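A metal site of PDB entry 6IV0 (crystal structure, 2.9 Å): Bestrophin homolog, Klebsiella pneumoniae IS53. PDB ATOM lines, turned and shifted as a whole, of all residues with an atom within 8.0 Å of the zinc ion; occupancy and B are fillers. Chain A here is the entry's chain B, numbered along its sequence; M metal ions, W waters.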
ATOM      1  N   VAL A  99       9.538  27.636   7.837  1.00  0.00           N
ATOM      2  CA  VAL A  99       8.847  27.595   6.557  1.00  0.00           C
ATOM      3  C   VAL A  99       9.239  28.810   5.738  1.00  0.00           C
ATOM      4  O   VAL A  99       9.470  28.697   4.534  1.00  0.00           O
ATOM      5  CB  VAL A  99       7.321  27.522   6.732  1.00  0.00           C
ATOM      6  CG1 VAL A  99       6.596  27.702   5.400  1.00  0.00           C
ATOM      7  CG2 VAL A  99       6.957  26.208   7.339  1.00  0.00           C
ATOM      8  N   LEU A 102      12.641  28.378   4.236  1.00  0.00           N
ATOM      9  CA  LEU A 102      12.572  27.428   3.104  1.00  0.00           C
ATOM     10  C   LEU A 102      11.956  28.053   1.854  1.00  0.00           C
ATOM     11  O   LEU A 102      12.500  27.895   0.768  1.00  0.00           O
ATOM     12  CB  LEU A 102      11.800  26.176   3.470  1.00  0.00           C
ATOM     13  CG  LEU A 102      12.599  25.266   4.402  1.00  0.00           C
ATOM     14  CD1 LEU A 102      11.632  24.343   5.122  1.00  0.00           C
ATOM     15  CD2 LEU A 102      13.670  24.478   3.677  1.00  0.00           C
ATOM     16  N   ARG A 103      10.861  28.782   2.004  1.00  0.00           N
ATOM     17  CA  ARG A 103      10.342  29.558   0.888  1.00  0.00           C
ATOM     18  C   ARG A 103      11.357  30.681   0.458  1.00  0.00           C
ATOM     19  O   ARG A 103      11.404  31.063  -0.709  1.00  0.00           O
ATOM     20  CB  ARG A 103       8.952  30.165   1.239  1.00  0.00           C
ATOM     21  CG  ARG A 103       7.853  29.140   1.614  1.00  0.00           C
ATOM     22  CD  ARG A 103       6.390  29.745   1.762  1.00  0.00           C
ATOM     23  NE  ARG A 103       5.406  28.913   2.517  1.00  0.00           N
ATOM     24  CZ  ARG A 103       4.678  27.899   2.039  1.00  0.00           C
ATOM     25  NH1 ARG A 103       3.824  27.243   2.810  1.00  0.00           N
ATOM     26  NH2 ARG A 103       4.829  27.487   0.788  1.00  0.00           N
ATOM     27  N   LEU A 106      15.113  28.288  -0.690  1.00  0.00           N
ATOM     28  CA  LEU A 106      14.830  27.262  -1.667  1.00  0.00           C
ATOM     29  C   LEU A 106      13.417  27.448  -2.208  1.00  0.00           C
ATOM     30  O   LEU A 106      12.580  26.570  -2.030  1.00  0.00           O
ATOM     31  CB  LEU A 106      14.971  25.881  -1.024  1.00  0.00           C
ATOM     32  CG  LEU A 106      16.348  25.574  -0.469  1.00  0.00           C
ATOM     33  CD1 LEU A 106      16.376  24.194   0.178  1.00  0.00           C
ATOM     34  CD2 LEU A 106      17.392  25.708  -1.572  1.00  0.00           C
ATOM     35  N   PRO A 107      13.142  28.605  -2.853  1.00  0.00           N
ATOM     36  CA  PRO A 107      11.778  28.940  -3.266  1.00  0.00           C
ATOM     37  C   PRO A 107      11.128  27.885  -4.138  1.00  0.00           C
ATOM     38  O   PRO A 107       9.908  27.754  -4.094  1.00  0.00           O
ATOM     39  CB  PRO A 107      11.940  30.230  -4.066  1.00  0.00           C
ATOM     40  CG  PRO A 107      13.349  30.280  -4.439  1.00  0.00           C
ATOM     41  CD  PRO A 107      14.095  29.644  -3.293  1.00  0.00           C
ATOM     42  N   ALA A 108      11.927  27.151  -4.904  1.00  0.00           N
ATOM     43  CA  ALA A 108      11.426  26.165  -5.864  1.00  0.00           C
ATOM     44  C   ALA A 108      11.018  24.824  -5.244  1.00  0.00           C
ATOM     45  O   ALA A 108      10.070  24.179  -5.689  1.00  0.00           O
ATOM     46  CB  ALA A 108      12.489  25.924  -6.941  1.00  0.00           C
ATOM     47  N   GLU A 109      11.752  24.425  -4.201  1.00  0.00           N
ATOM     48  CA  GLU A 109      11.692  23.080  -3.648  1.00  0.00           C
ATOM     49  C   GLU A 109      10.398  22.737  -2.911  1.00  0.00           C
ATOM     50  O   GLU A 109      10.446  22.428  -1.714  1.00  0.00           O
ATOM     51  CB  GLU A 109      12.876  22.908  -2.707  1.00  0.00           C
ATOM     52  CG  GLU A 109      14.233  22.902  -3.406  1.00  0.00           C
ATOM     53  CD  GLU A 109      14.567  21.556  -4.041  1.00  0.00           C
ATOM     54  OE1 GLU A 109      13.861  20.549  -3.739  1.00  0.00           O
ATOM     55  OE2 GLU A 109      15.528  21.506  -4.847  1.00  0.00           O
ATOM     56  N   HIS A 110       9.261  22.718  -3.617  1.00  0.00           N
ATOM     57  CA  HIS A 110       7.953  22.596  -2.943  1.00  0.00           C
ATOM     58  C   HIS A 110       7.628  21.215  -2.389  1.00  0.00           C
ATOM     59  O   HIS A 110       6.691  21.067  -1.604  1.00  0.00           O
ATOM     60  CB  HIS A 110       6.804  23.003  -3.868  1.00  0.00           C
ATOM     61  CG  HIS A 110       6.908  24.394  -4.391  1.00  0.00           C
ATOM     62  ND1 HIS A 110       7.130  25.490  -3.582  1.00  0.00           N
ATOM     63  CD2 HIS A 110       6.808  24.869  -5.661  1.00  0.00           C
ATOM     64  CE1 HIS A 110       7.180  26.580  -4.337  1.00  0.00           C
ATOM     65  NE2 HIS A 110       6.987  26.229  -5.590  1.00  0.00           N
ATOM     66  N   ASP A 111       8.364  20.186  -2.793  1.00  0.00           N
ATOM     67  CA  ASP A 111       8.023  18.871  -2.263  1.00  0.00           C
ATOM     68  C   ASP A 111       8.797  18.642  -0.995  1.00  0.00           C
ATOM     69  O   ASP A 111       8.400  17.821  -0.159  1.00  0.00           O
ATOM     70  CB  ASP A 111       8.282  17.755  -3.300  1.00  0.00           C
ATOM     71  CG  ASP A 111       7.041  17.471  -4.158  1.00  0.00           C
ATOM     72  OD1 ASP A 111       6.052  16.952  -3.598  1.00  0.00           O
ATOM     73  OD2 ASP A 111       7.062  17.744  -5.381  1.00  0.00           O
ATOM     74  N   ALA A 112       9.893  19.377  -0.828  1.00  0.00           N
ATOM     75  CA  ALA A 112      10.571  19.447   0.462  1.00  0.00           C
ATOM     76  C   ALA A 112       9.727  20.322   1.382  1.00  0.00           C
ATOM     77  O   ALA A 112       9.482  19.930   2.525  1.00  0.00           O
ATOM     78  CB  ALA A 112      11.975  19.995   0.311  1.00  0.00           C
ATOM     79  N   HIS A 113       9.264  21.467   0.869  1.00  0.00           N
ATOM     80  CA  HIS A 113       8.347  22.349   1.619  1.00  0.00           C
ATOM     81  C   HIS A 113       7.173  21.592   2.227  1.00  0.00           C
ATOM     82  O   HIS A 113       6.875  21.763   3.408  1.00  0.00           O
ATOM     83  CB  HIS A 113       7.778  23.451   0.722  1.00  0.00           C
ATOM     84  CG  HIS A 113       8.798  24.411   0.221  1.00  0.00           C
ATOM     85  ND1 HIS A 113       8.532  25.309  -0.798  1.00  0.00           N
ATOM     86  CD2 HIS A 113      10.091  24.620   0.575  1.00  0.00           C
ATOM     87  CE1 HIS A 113       9.623  26.022  -1.043  1.00  0.00           C
ATOM     88  NE2 HIS A 113      10.576  25.618  -0.223  1.00  0.00           N
ATOM     89  N   ARG A 114       6.508  20.772   1.407  1.00  0.00           N
ATOM     90  CA  ARG A 114       5.339  20.023   1.852  1.00  0.00           C
ATOM     91  C   ARG A 114       5.695  19.005   2.921  1.00  0.00           C
ATOM     92  O   ARG A 114       4.988  18.878   3.925  1.00  0.00           O
ATOM     93  CB  ARG A 114       4.654  19.304   0.683  1.00  0.00           C
ATOM     94  CG  ARG A 114       3.452  20.058   0.151  1.00  0.00           C
ATOM     95  CD  ARG A 114       2.544  19.181  -0.723  1.00  0.00           C
ATOM     96  NE  ARG A 114       3.257  18.618  -1.875  1.00  0.00           N
ATOM     97  CZ  ARG A 114       3.468  19.268  -3.026  1.00  0.00           C
ATOM     98  NH1 ARG A 114       3.030  20.520  -3.185  1.00  0.00           N
ATOM     99  NH2 ARG A 114       4.124  18.658  -4.000  1.00  0.00           N
ATOM    100  N   VAL A 117       6.582  20.781   6.317  1.00  0.00           N
ATOM    101  CA  VAL A 117       5.387  21.341   6.945  1.00  0.00           C
ATOM    102  C   VAL A 117       4.505  20.294   7.619  1.00  0.00           C
ATOM    103  O   VAL A 117       3.843  20.566   8.621  1.00  0.00           O
ATOM    104  CB  VAL A 117       4.547  22.127   5.931  1.00  0.00           C
ATOM    105  CG1 VAL A 117       3.163  22.459   6.497  1.00  0.00           C
ATOM    106  CG2 VAL A 117       5.258  23.403   5.528  1.00  0.00           C
ATOM    107  N   THR A 289      -3.374  26.678   1.241  1.00  0.00           N
ATOM    108  CA  THR A 289      -2.889  25.406   0.653  1.00  0.00           C
ATOM    109  C   THR A 289      -1.382  25.437   0.298  1.00  0.00           C
ATOM    110  O   THR A 289      -0.975  24.904  -0.734  1.00  0.00           O
ATOM    111  CB  THR A 289      -3.673  24.981  -0.629  1.00  0.00           C
ATOM    112  OG1 THR A 289      -3.399  25.888  -1.704  1.00  0.00           O
ATOM    113  CG2 THR A 289      -5.201  24.907  -0.364  1.00  0.00           C
ATOM    114  N   GLY A 290      -0.573  26.077   1.149  1.00  0.00           N
ATOM    115  CA  GLY A 290       0.874  26.040   1.020  1.00  0.00           C
ATOM    116  C   GLY A 290       1.449  26.854  -0.123  1.00  0.00           C
ATOM    117  O   GLY A 290       2.600  26.617  -0.496  1.00  0.00           O
ATOM    118  N   GLN A 291       0.684  27.808  -0.649  1.00  0.00           N
ATOM    119  CA  GLN A 291       1.127  28.679  -1.755  1.00  0.00           C
ATOM    120  C   GLN A 291       1.673  30.061  -1.321  1.00  0.00           C
ATOM    121  O   GLN A 291       1.133  30.686  -0.392  1.00  0.00           O
ATOM    122  CB  GLN A 291      -0.010  28.883  -2.757  1.00  0.00           C
ATOM    123  CG  GLN A 291       0.193  30.073  -3.704  1.00  0.00           C
ATOM    124  CD  GLN A 291      -0.943  30.310  -4.680  1.00  0.00           C
ATOM    125  OE1 GLN A 291      -2.010  29.690  -4.590  1.00  0.00           O
ATOM    126  NE2 GLN A 291      -0.721  31.210  -5.646  1.00  0.00           N
ATOM    127  N   HIS A 292       2.692  30.546  -2.039  1.00  0.00           N
ATOM    128  CA  HIS A 292       3.426  31.740  -1.632  1.00  0.00           C
ATOM    129  C   HIS A 292       3.815  32.601  -2.855  1.00  0.00           C
ATOM    130  O   HIS A 292       3.906  32.082  -3.966  1.00  0.00           O
ATOM    131  CB  HIS A 292       4.668  31.329  -0.783  1.00  0.00           C
ATOM    132  CG  HIS A 292       5.463  30.156  -1.316  1.00  0.00           C
ATOM    133  ND1 HIS A 292       6.838  30.213  -1.476  1.00  0.00           N
ATOM    134  CD2 HIS A 292       5.091  28.931  -1.800  1.00  0.00           C
ATOM    135  CE1 HIS A 292       7.278  29.062  -1.952  1.00  0.00           C
ATOM    136  NE2 HIS A 292       6.237  28.263  -2.155  1.00  0.00           N
HETATM  137 ZN    ZN M   1       6.549  25.799  -1.587  1.00  0.00          ZN
HETATM  138  O   HOH W   1       4.629  24.526  -0.751  1.00  0.00           O
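The backbone carbonyl oxygen of Leu 106 is in hydrogen-bond range of a ring nitrogen (NE2) of His 113 (2.9 Å).
NE2 of His 113 sits at hydrogen-bond distance from O of Leu 102, 3.1 Å away.
The guanidinium group of Arg 103 sits close to a ring nitrogen (NE2) of His 292 (3.4 Å).
The guanidinium group of Arg 103 is in hydrogen-bond range of the backbone carbonyl oxygen of Gly 290 (2.7 Å).
Residues that only touch the zinc ion: Arg 103 (3.4 Å).
Of the 17 residues printed, 4 come within 4 Å of the zinc ion.
Along chain A the residues within 4 Å of the zinc ion span positions 103 to 292.
ND1 of His 110 is bound to the zinc ion (2.1 Å).
A ring nitrogen (ND1) of His 113 binds the zinc ion (2.2 Å).
Water W1 is bound to the zinc ion (2.5 Å).
The zinc ion is bound by NE2 of His 292 (2.5 Å).
Water W1 bridges the backbone carbonyl oxygen of Gly 290 (2.9 Å) and the guanidinium group of Arg 103 (3.3 Å).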
